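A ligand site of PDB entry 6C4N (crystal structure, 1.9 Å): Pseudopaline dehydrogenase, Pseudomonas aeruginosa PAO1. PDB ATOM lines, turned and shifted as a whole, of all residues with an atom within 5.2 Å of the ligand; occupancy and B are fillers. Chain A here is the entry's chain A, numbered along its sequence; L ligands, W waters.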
ATOM      1  N   GLY A  31      13.144  28.389  -0.577  1.00  0.00           N
ATOM      2  CA  GLY A  31      13.671  27.232   0.108  1.00  0.00           C
ATOM      3  C   GLY A  31      14.456  26.440  -0.909  1.00  0.00           C
ATOM      4  O   GLY A  31      13.913  26.112  -1.967  1.00  0.00           O
ATOM      5  N   LEU A  32      15.726  26.182  -0.671  1.00  0.00           N
ATOM      6  CA  LEU A  32      16.556  25.428  -1.604  1.00  0.00           C
ATOM      7  C   LEU A  32      17.110  24.195  -0.908  1.00  0.00           C
ATOM      8  O   LEU A  32      18.306  24.107  -0.600  1.00  0.00           O
ATOM      9  CB  LEU A  32      17.669  26.346  -2.189  1.00  0.00           C
ATOM     10  CG  LEU A  32      18.523  25.769  -3.323  1.00  0.00           C
ATOM     11  CD1 LEU A  32      17.687  25.143  -4.429  1.00  0.00           C
ATOM     12  CD2 LEU A  32      19.420  26.856  -3.914  1.00  0.00           C
ATOM     13  N   GLY A  33      16.221  23.217  -0.664  1.00  0.00           N
ATOM     14  CA  GLY A  33      16.596  21.947  -0.080  1.00  0.00           C
ATOM     15  C   GLY A  33      16.311  20.789  -1.015  1.00  0.00           C
ATOM     16  O   GLY A  33      16.298  20.988  -2.240  1.00  0.00           O
ATOM     17  N   ALA A  34      16.053  19.597  -0.472  1.00  0.00           N
ATOM     18  CA  ALA A  34      15.947  18.413  -1.312  1.00  0.00           C
ATOM     19  C   ALA A  34      14.811  18.559  -2.313  1.00  0.00           C
ATOM     20  O   ALA A  34      14.998  18.338  -3.519  1.00  0.00           O
ATOM     21  CB  ALA A  34      15.747  17.160  -0.450  1.00  0.00           C
ATOM     22  N   VAL A  35      13.633  18.977  -1.853  1.00  0.00           N
ATOM     23  CA  VAL A  35      12.493  19.109  -2.753  1.00  0.00           C
ATOM     24  C   VAL A  35      12.811  20.081  -3.885  1.00  0.00           C
ATOM     25  O   VAL A  35      12.541  19.799  -5.062  1.00  0.00           O
ATOM     26  CB  VAL A  35      11.260  19.559  -1.947  1.00  0.00           C
ATOM     27  CG1 VAL A  35      10.180  20.129  -2.842  1.00  0.00           C
ATOM     28  CG2 VAL A  35      10.691  18.395  -1.183  1.00  0.00           C
ATOM     29  N   ALA A  36      13.426  21.225  -3.546  1.00  0.00           N
ATOM     30  CA  ALA A  36      13.669  22.270  -4.533  1.00  0.00           C
ATOM     31  C   ALA A  36      14.561  21.789  -5.655  1.00  0.00           C
ATOM     32  O   ALA A  36      14.408  22.200  -6.816  1.00  0.00           O
ATOM     33  CB  ALA A  36      14.291  23.515  -3.867  1.00  0.00           C
ATOM     34  N   ASN A  55      16.695  31.495  -0.015  1.00  0.00           N
ATOM     35  CA  ASN A  55      16.780  30.682   1.191  1.00  0.00           C
ATOM     36  C   ASN A  55      17.325  31.543   2.325  1.00  0.00           C
ATOM     37  O   ASN A  55      18.298  32.277   2.145  1.00  0.00           O
ATOM     38  CB  ASN A  55      17.677  29.484   0.976  1.00  0.00           C
ATOM     39  CG  ASN A  55      17.409  28.404   1.978  1.00  0.00           C
ATOM     40  OD1 ASN A  55      16.316  27.866   2.020  1.00  0.00           O
ATOM     41  ND2 ASN A  55      18.385  28.124   2.830  1.00  0.00           N
ATOM     42  N   HIS A  56      16.680  31.465   3.479  1.00  0.00           N
ATOM     43  CA  HIS A  56      17.016  32.380   4.571  1.00  0.00           C
ATOM     44  C   HIS A  56      18.435  32.123   5.086  1.00  0.00           C
ATOM     45  O   HIS A  56      18.995  31.045   4.858  1.00  0.00           O
ATOM     46  CB  HIS A  56      15.985  32.256   5.704  1.00  0.00           C
ATOM     47  CG  HIS A  56      15.948  30.913   6.403  1.00  0.00           C
ATOM     48  ND1 HIS A  56      15.222  30.716   7.561  1.00  0.00           N
ATOM     49  CD2 HIS A  56      16.512  29.718   6.111  1.00  0.00           C
ATOM     50  CE1 HIS A  56      15.369  29.465   7.966  1.00  0.00           C
ATOM     51  NE2 HIS A  56      16.159  28.846   7.111  1.00  0.00           N
ATOM     52  N   PRO A  57      19.033  33.110   5.776  1.00  0.00           N
ATOM     53  CA  PRO A  57      20.445  32.980   6.185  1.00  0.00           C
ATOM     54  C   PRO A  57      20.701  31.793   7.100  1.00  0.00           C
ATOM     55  O   PRO A  57      19.825  31.331   7.821  1.00  0.00           O
ATOM     56  CB  PRO A  57      20.720  34.310   6.912  1.00  0.00           C
ATOM     57  CG  PRO A  57      19.780  35.290   6.286  1.00  0.00           C
ATOM     58  CD  PRO A  57      18.507  34.461   6.058  1.00  0.00           C
ATOM     59  N   GLY A  58      21.927  31.321   7.050  1.00  0.00           N
ATOM     60  CA  GLY A  58      22.342  30.178   7.826  1.00  0.00           C
ATOM     61  C   GLY A  58      23.458  29.430   7.116  1.00  0.00           C
ATOM     62  O   GLY A  58      23.896  29.803   6.029  1.00  0.00           O
ATOM     63  N   ARG A  60      23.461  26.579   5.637  1.00  0.00           N
ATOM     64  CA  ARG A  60      23.087  25.994   4.363  1.00  0.00           C
ATOM     65  C   ARG A  60      23.183  27.026   3.250  1.00  0.00           C
ATOM     66  O   ARG A  60      23.783  26.753   2.207  1.00  0.00           O
ATOM     67  CB  ARG A  60      21.669  25.402   4.420  1.00  0.00           C
ATOM     68  CG  ARG A  60      21.296  24.691   3.081  1.00  0.00           C
ATOM     69  CD  ARG A  60      20.065  23.772   3.154  1.00  0.00           C
ATOM     70  NE  ARG A  60      19.757  23.443   1.761  1.00  0.00           N
ATOM     71  CZ  ARG A  60      20.401  22.502   1.057  1.00  0.00           C
ATOM     72  NH1 ARG A  60      20.076  22.297  -0.199  1.00  0.00           N
ATOM     73  NH2 ARG A  60      21.353  21.749   1.590  1.00  0.00           N
ATOM     74  N   SER A  61      22.610  28.208   3.463  1.00  0.00           N
ATOM     75  CA  SER A  61      22.690  29.270   2.461  1.00  0.00           C
ATOM     76  C   SER A  61      24.120  29.685   2.210  1.00  0.00           C
ATOM     77  O   SER A  61      24.486  30.018   1.082  1.00  0.00           O
ATOM     78  CB  SER A  61      21.878  30.487   2.888  1.00  0.00           C
ATOM     79  OG  SER A  61      20.496  30.252   2.744  1.00  0.00           O
ATOM     80  N   CYS A 111       9.178  25.570  -1.453  1.00  0.00           N
ATOM     81  CA  CYS A 111       9.848  24.323  -1.140  1.00  0.00           C
ATOM     82  C   CYS A 111      10.334  24.257   0.293  1.00  0.00           C
ATOM     83  O   CYS A 111      11.170  23.419   0.611  1.00  0.00           O
ATOM     84  CB  CYS A 111      11.015  24.140  -2.082  1.00  0.00           C
ATOM     85  SG  CYS A 111      10.430  24.161  -3.856  1.00  0.00           S
ATOM     86  N   VAL A 112       9.893  25.181   1.130  1.00  0.00           N
ATOM     87  CA  VAL A 112      10.172  25.161   2.552  1.00  0.00           C
ATOM     88  C   VAL A 112       9.292  24.127   3.239  1.00  0.00           C
ATOM     89  O   VAL A 112       8.370  23.568   2.622  1.00  0.00           O
ATOM     90  CB  VAL A 112       9.948  26.560   3.143  1.00  0.00           C
ATOM     91  CG1 VAL A 112      10.927  27.531   2.559  1.00  0.00           C
ATOM     92  CG2 VAL A 112       8.493  26.992   2.895  1.00  0.00           C
ATOM     93  N   PRO A 113       9.518  23.833   4.518  1.00  0.00           N
ATOM     94  CA  PRO A 113       8.614  22.937   5.222  1.00  0.00           C
ATOM     95  C   PRO A 113       7.221  23.542   5.302  1.00  0.00           C
ATOM     96  O   PRO A 113       7.047  24.753   5.475  1.00  0.00           O
ATOM     97  CB  PRO A 113       9.245  22.793   6.615  1.00  0.00           C
ATOM     98  CG  PRO A 113      10.695  23.084   6.387  1.00  0.00           C
ATOM     99  CD  PRO A 113      10.717  24.141   5.311  1.00  0.00           C
ATOM    100  N   ALA A 114       6.207  22.675   5.191  1.00  0.00           N
ATOM    101  CA  ALA A 114       4.842  23.165   5.133  1.00  0.00           C
ATOM    102  C   ALA A 114       4.442  23.926   6.405  1.00  0.00           C
ATOM    103  O   ALA A 114       3.622  24.848   6.333  1.00  0.00           O
ATOM    104  CB  ALA A 114       3.881  22.003   4.848  1.00  0.00           C
ATOM    105  N   SER A 116       6.130  26.032   7.881  1.00  0.00           N
ATOM    106  CA  SER A 116       6.666  27.398   7.806  1.00  0.00           C
ATOM    107  C   SER A 116       6.002  28.271   6.735  1.00  0.00           C
ATOM    108  O   SER A 116       6.406  29.419   6.542  1.00  0.00           O
ATOM    109  CB  SER A 116       8.171  27.341   7.529  1.00  0.00           C
ATOM    110  OG  SER A 116       8.405  27.001   6.173  1.00  0.00           O
ATOM    111  N   VAL A 120       6.945  32.159   6.011  1.00  0.00           N
ATOM    112  CA  VAL A 120       7.690  32.430   4.798  1.00  0.00           C
ATOM    113  C   VAL A 120       6.919  33.395   3.935  1.00  0.00           C
ATOM    114  O   VAL A 120       7.489  34.348   3.372  1.00  0.00           O
ATOM    115  CB  VAL A 120       8.018  31.097   4.092  1.00  0.00           C
ATOM    116  CG1 VAL A 120       8.465  31.295   2.671  1.00  0.00           C
ATOM    117  CG2 VAL A 120       9.103  30.396   4.852  1.00  0.00           C
ATOM    118  N   SER A 139       3.819  20.950  -0.710  1.00  0.00           N
ATOM    119  CA  SER A 139       3.386  19.928   0.265  1.00  0.00           C
ATOM    120  C   SER A 139       2.266  20.533   1.102  1.00  0.00           C
ATOM    121  O   SER A 139       2.441  20.931   2.244  1.00  0.00           O
ATOM    122  CB  SER A 139       4.564  19.462   1.135  1.00  0.00           C
ATOM    123  OG  SER A 139       4.137  18.521   2.126  1.00  0.00           O
ATOM    124  N   TYR A 166       4.365  16.262  -1.767  1.00  0.00           N
ATOM    125  CA  TYR A 166       5.574  16.183  -2.567  1.00  0.00           C
ATOM    126  C   TYR A 166       5.562  14.838  -3.279  1.00  0.00           C
ATOM    127  O   TYR A 166       5.146  13.837  -2.719  1.00  0.00           O
ATOM    128  CB  TYR A 166       6.818  16.314  -1.710  1.00  0.00           C
ATOM    129  CG  TYR A 166       8.079  16.125  -2.500  1.00  0.00           C
ATOM    130  CD1 TYR A 166       8.325  16.865  -3.625  1.00  0.00           C
ATOM    131  CD2 TYR A 166       9.012  15.171  -2.127  1.00  0.00           C
ATOM    132  CE1 TYR A 166       9.461  16.690  -4.363  1.00  0.00           C
ATOM    133  CE2 TYR A 166      10.167  14.984  -2.856  1.00  0.00           C
ATOM    134  CZ  TYR A 166      10.389  15.759  -3.980  1.00  0.00           C
ATOM    135  OH  TYR A 166      11.543  15.571  -4.719  1.00  0.00           O
ATOM    136  N   ALA A 168       7.880  12.751  -4.609  1.00  0.00           N
ATOM    137  CA  ALA A 168       8.974  11.806  -4.614  1.00  0.00           C
ATOM    138  C   ALA A 168       9.464  11.607  -3.195  1.00  0.00           C
ATOM    139  O   ALA A 168       8.848  12.060  -2.229  1.00  0.00           O
ATOM    140  CB  ALA A 168      10.058  12.308  -5.580  1.00  0.00           C
ATOM    141  N   ALA A 169      10.581  10.891  -3.062  1.00  0.00           N
ATOM    142  CA  ALA A 169      11.330  10.849  -1.816  1.00  0.00           C
ATOM    143  C   ALA A 169      12.741  11.228  -2.195  1.00  0.00           C
ATOM    144  O   ALA A 169      13.361  10.559  -3.030  1.00  0.00           O
ATOM    145  CB  ALA A 169      11.313   9.469  -1.158  1.00  0.00           C
ATOM    146  N   THR A 170      13.227  12.320  -1.599  1.00  0.00           N
ATOM    147  CA  THR A 170      14.467  12.961  -2.032  1.00  0.00           C
ATOM    148  C   THR A 170      15.198  13.450  -0.799  1.00  0.00           C
ATOM    149  O   THR A 170      14.560  13.975   0.115  1.00  0.00           O
ATOM    150  CB  THR A 170      14.150  14.158  -2.961  1.00  0.00           C
ATOM    151  OG1 THR A 170      13.285  13.725  -3.992  1.00  0.00           O
ATOM    152  CG2 THR A 170      15.398  14.765  -3.575  1.00  0.00           C
ATOM    153  N   LYS A 171      16.527  13.280  -0.772  1.00  0.00           N
ATOM    154  CA  LYS A 171      17.275  13.958   0.279  1.00  0.00           C
ATOM    155  C   LYS A 171      18.636  14.400  -0.218  1.00  0.00           C
ATOM    156  O   LYS A 171      19.169  13.898  -1.213  1.00  0.00           O
ATOM    157  CB  LYS A 171      17.412  13.119   1.552  1.00  0.00           C
ATOM    158  CG  LYS A 171      18.077  11.817   1.465  1.00  0.00           C
ATOM    159  CD  LYS A 171      18.048  11.230   2.873  1.00  0.00           C
ATOM    160  CE  LYS A 171      18.334   9.739   2.923  1.00  0.00           C
ATOM    161  NZ  LYS A 171      17.999   9.181   4.279  1.00  0.00           N
ATOM    162  N   VAL A 172      19.166  15.408   0.458  1.00  0.00           N
ATOM    163  CA  VAL A 172      20.515  15.897   0.191  1.00  0.00           C
ATOM    164  C   VAL A 172      21.439  14.938   0.928  1.00  0.00           C
ATOM    165  O   VAL A 172      21.417  14.877   2.151  1.00  0.00           O
ATOM    166  CB  VAL A 172      20.698  17.341   0.680  1.00  0.00           C
ATOM    167  CG1 VAL A 172      22.157  17.781   0.586  1.00  0.00           C
ATOM    168  CG2 VAL A 172      19.809  18.291  -0.110  1.00  0.00           C
ATOM    169  N   THR A 231       1.225  12.525   4.128  1.00  0.00           N
ATOM    170  CA  THR A 231       1.878  12.545   5.440  1.00  0.00           C
ATOM    171  C   THR A 231       0.895  12.869   6.559  1.00  0.00           C
ATOM    172  O   THR A 231       1.053  12.341   7.664  1.00  0.00           O
ATOM    173  CB  THR A 231       3.069  13.529   5.478  1.00  0.00           C
ATOM    174  OG1 THR A 231       2.712  14.800   4.963  1.00  0.00           O
ATOM    175  CG2 THR A 231       4.196  13.005   4.656  1.00  0.00           C
ATOM    176  N   ARG A 376      11.932  17.257  11.612  1.00  0.00           N
ATOM    177  CA  ARG A 376      10.657  17.531  10.961  1.00  0.00           C
ATOM    178  C   ARG A 376       9.633  16.458  11.263  1.00  0.00           C
ATOM    179  O   ARG A 376       8.448  16.739  11.468  1.00  0.00           O
ATOM    180  CB  ARG A 376      10.839  17.667   9.438  1.00  0.00           C
ATOM    181  CG  ARG A 376      10.887  19.100   8.905  1.00  0.00           C
ATOM    182  CD  ARG A 376      11.659  20.072   9.850  1.00  0.00           C
ATOM    183  NE  ARG A 376      11.231  21.468   9.668  1.00  0.00           N
ATOM    184  CZ  ARG A 376      10.283  22.076  10.377  1.00  0.00           C
ATOM    185  NH1 ARG A 376       9.644  21.436  11.355  1.00  0.00           N
ATOM    186  NH2 ARG A 376       9.990  23.342  10.137  1.00  0.00           N
ATOM    187  N   GLU A 380       7.003  19.073  12.369  1.00  0.00           N
ATOM    188  CA  GLU A 380       6.122  19.484  11.281  1.00  0.00           C
ATOM    189  C   GLU A 380       4.811  18.709  11.315  1.00  0.00           C
ATOM    190  O   GLU A 380       3.734  19.282  11.124  1.00  0.00           O
ATOM    191  CB  GLU A 380       6.825  19.307   9.941  1.00  0.00           C
ATOM    192  CG  GLU A 380       5.872  19.429   8.753  1.00  0.00           C
ATOM    193  CD  GLU A 380       6.595  19.430   7.383  1.00  0.00           C
ATOM    194  OE1 GLU A 380       5.935  19.735   6.368  1.00  0.00           O
ATOM    195  OE2 GLU A 380       7.813  19.142   7.326  1.00  0.00           O
HETATM  196  P1  LIG L   1      14.937  20.538   3.448  1.00  0.00           P
HETATM  197  O1  LIG L   1      15.798  19.693   2.597  1.00  0.00           O
HETATM  198  O2  LIG L   1      15.225  20.498   4.900  1.00  0.00           O
HETATM  199  O3  LIG L   1      15.015  22.139   2.925  1.00  0.00           O
HETATM  200  C1  LIG L   1      13.953  22.964   2.730  1.00  0.00           C
HETATM  201  C2  LIG L   1      14.541  24.401   2.636  1.00  0.00           C
HETATM  202  O4  LIG L   1      13.825  25.282   3.331  1.00  0.00           O
HETATM  203  C3  LIG L   1      15.973  24.481   3.195  1.00  0.00           C
HETATM  204  O5  LIG L   1      16.742  25.132   2.274  1.00  0.00           O
HETATM  205  C4  LIG L   1      15.828  25.262   4.532  1.00  0.00           C
HETATM  206  O6  LIG L   1      17.119  25.948   4.795  1.00  0.00           O
HETATM  207  C5  LIG L   1      14.764  26.050   4.390  1.00  0.00           C
HETATM  208  N1  LIG L   1      13.967  26.156   5.631  1.00  0.00           N
HETATM  209  C6  LIG L   1      13.706  25.296   6.601  1.00  0.00           C
HETATM  210  N2  LIG L   1      12.919  25.899   7.517  1.00  0.00           N
HETATM  211  C7  LIG L   1      12.676  27.136   7.102  1.00  0.00           C
HETATM  212  C8  LIG L   1      11.941  28.154   7.651  1.00  0.00           C
HETATM  213  N3  LIG L   1      11.225  28.041   8.874  1.00  0.00           N
HETATM  214  N4  LIG L   1      11.824  29.345   7.025  1.00  0.00           N
HETATM  215  C9  LIG L   1      12.475  29.524   5.865  1.00  0.00           C
HETATM  216  N5  LIG L   1      13.191  28.509   5.318  1.00  0.00           N
HETATM  217  C10 LIG L   1      13.294  27.309   5.926  1.00  0.00           C
HETATM  218  O7  LIG L   1      13.393  20.042   3.393  1.00  0.00           O
HETATM  219  P2  LIG L   1      12.855  19.153   2.159  1.00  0.00           P
HETATM  220  O8  LIG L   1      13.284  17.751   2.251  1.00  0.00           O
HETATM  221  O9  LIG L   1      13.217  19.789   0.826  1.00  0.00           O
HETATM  222  O10 LIG L   1      11.269  19.172   2.406  1.00  0.00           O
HETATM  223  C11 LIG L   1      10.460  20.325   2.322  1.00  0.00           C
HETATM  224  C12 LIG L   1       9.052  19.847   2.604  1.00  0.00           C
HETATM  225  O11 LIG L   1       8.613  18.941   1.703  1.00  0.00           O
HETATM  226  C13 LIG L   1       9.111  19.031   3.863  1.00  0.00           C
HETATM  227  O12 LIG L   1       8.972  19.893   4.884  1.00  0.00           O
HETATM  228  C14 LIG L   1       7.794  18.220   3.789  1.00  0.00           C
HETATM  229  O13 LIG L   1       6.845  19.316   4.185  1.00  0.00           O
HETATM  230  C15 LIG L   1       7.700  17.882   2.526  1.00  0.00           C
HETATM  231  N6  LIG L   1       8.164  16.507   2.171  1.00  0.00           N
HETATM  232  C16 LIG L   1       9.421  16.255   1.676  1.00  0.00           C
HETATM  233  C17 LIG L   1       9.786  14.949   1.338  1.00  0.00           C
HETATM  234  C18 LIG L   1      11.179  14.570   0.805  1.00  0.00           C
HETATM  235  O14 LIG L   1      11.352  13.479   0.274  1.00  0.00           O
HETATM  236  N7  LIG L   1      12.265  15.426   0.940  1.00  0.00           N
HETATM  237  C19 LIG L   1       8.885  13.957   1.483  1.00  0.00           C
HETATM  238  C20 LIG L   1       7.636  14.205   1.947  1.00  0.00           C
HETATM  239  C21 LIG L   1       7.277  15.490   2.296  1.00  0.00           C
HETATM  240  P3  LIG L   1      17.780  25.814   6.285  1.00  0.00           P
HETATM  241  O15 LIG L   1      18.969  26.709   6.357  1.00  0.00           O
HETATM  242  O16 LIG L   1      16.697  26.245   7.207  1.00  0.00           O
HETATM  243  O17 LIG L   1      18.139  24.422   6.494  1.00  0.00           O
HETATM  244  O   HOH W   1      10.946  31.855   8.093  1.00  0.00           O
HETATM  245  O   HOH W   2      20.582  28.713   5.522  1.00  0.00           O
HETATM  246  O   HOH W   3       3.959  15.645   1.511  1.00  0.00           O
HETATM  247  O   HOH W   4      10.090  30.444  10.124  1.00  0.00           O
HETATM  248  O   HOH W   5      12.473  11.173   1.818  1.00  0.00           O
HETATM  249  O   HOH W   6      13.501  22.207  -0.520  1.00  0.00           O
HETATM  250  O   HOH W   7      21.197  26.000   7.588  1.00  0.00           O
HETATM  251  O   HOH W   8      15.041  16.046   3.312  1.00  0.00           O
HETATM  252  O   HOH W   9      15.454  22.313   6.736  1.00  0.00           O
HETATM  253  O   HOH W  10       5.019  13.165   0.141  1.00  0.00           O
HETATM  254  O   HOH W  11      19.182  28.703   8.558  1.00  0.00           O
HETATM  255  O   HOH W  12       4.475  17.735   4.945  1.00  0.00           O
HETATM  256  O   HOH W  13      13.855  30.308   3.098  1.00  0.00           O
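Residues that only touch the ligand: Pro 113, Ala 169, Gly 33, Ser 116, Cys 111, Tyr 166, Ala 114, Val 120, Val 112, Gly 31 and Ala 168.
Hydrophobic or aromatic side chains within 4 Å of the ligand: Ala 34, Val 35, His 56, Val 112, Pro 113, Val 120 and Tyr 166.
Of the 28 residues printed, 20 come within 4 Å of the ligand.
OE1 of Glu 380 lies within hydrogen-bond range of N of Ala 114, 3.2 Å away.
The side-chain hydroxyl of Ser 61 sits at hydrogen-bond distance from the side-chain amide nitrogen of Asn 55, at 3.0 Å.
The backbone carbonyl oxygen (O) of Pro 113 is in hydrogen-bond range of the side-chain hydroxyl (OG) of Ser 116 (2.7 Å).
OG1 of Thr 170 is in hydrogen-bond range of OH of Tyr 166 (2.6 Å).
The side-chain amide oxygen (OD1) of Asn 55 sits at hydrogen-bond distance from the backbone NH (N) of Leu 32 (3.2 Å).
The backbone carbonyl oxygen of His 56 sits at hydrogen-bond distance from the side-chain hydroxyl of Ser 61, at 2.7 Å.
NH1 of Arg 60 is in hydrogen-bond range of O of Leu 32, 2.6 Å away.
Water W7 bridges an oxygen (O15) of the ligand (2.6 Å) and the backbone NH (N) of Arg 60 (3.0 Å).
Water W2 lies within hydrogen-bond range of O15 of the ligand (2.7 Å), O of His 56 (2.9 Å), N of Ser 61 (2.9 Å) and N of Gly 58 (3.3 Å).
Water W13 bridges N5 of the ligand and N of His 56.
Water W12 lies within hydrogen-bond range of OE1 of Glu 380 (2.9 Å), OG of Ser 139 (2.9 Å), O13 of the ligand (2.9 Å) and OG1 of Thr 231 (3.4 Å).
Water W11 lies within hydrogen-bond range of the backbone carbonyl oxygen (O) of Pro 57 (2.8 Å), an oxygen (O15) of the ligand (3.0 Å) and a ring nitrogen (NE2) of His 56 (3.4 Å).
Water W3 lies within hydrogen-bond range of OG of Ser 139 (2.9 Å) and N of Tyr 166 (3.4 Å).
O16 of the ligand is in hydrogen-bond range of NE2 of His 56 (2.7 Å).
N of Ala 34 lies within hydrogen-bond range of O1 of the ligand.
An oxygen (O13) of the ligand lies within hydrogen-bond range of the side-chain carboxylate of Glu 380.
O5 of the ligand lies within hydrogen-bond range of NE of Arg 60 (3.5 Å).
N of Leu 32 lies within hydrogen-bond range of O5 of the ligand, 3.3 Å away.
O of Thr 170 is in hydrogen-bond range of N7 of the ligand, 2.8 Å away.
The backbone NH of Val 35 sits at hydrogen-bond distance from an oxygen (O9) of the ligand.
The side-chain hydroxyl (OG) of Ser 139 sits at hydrogen-bond distance from an oxygen (O13) of the ligand (3.5 Å).
O14 of the ligand lies within hydrogen-bond range of N of Thr 170 (2.9 Å).
O5 of the ligand lies close to O of Leu 32, 3.4 Å away.
The side-chain amide oxygen (OD1) of Asn 55 sits at hydrogen-bond distance from an oxygen (O5) of the ligand (2.8 Å).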
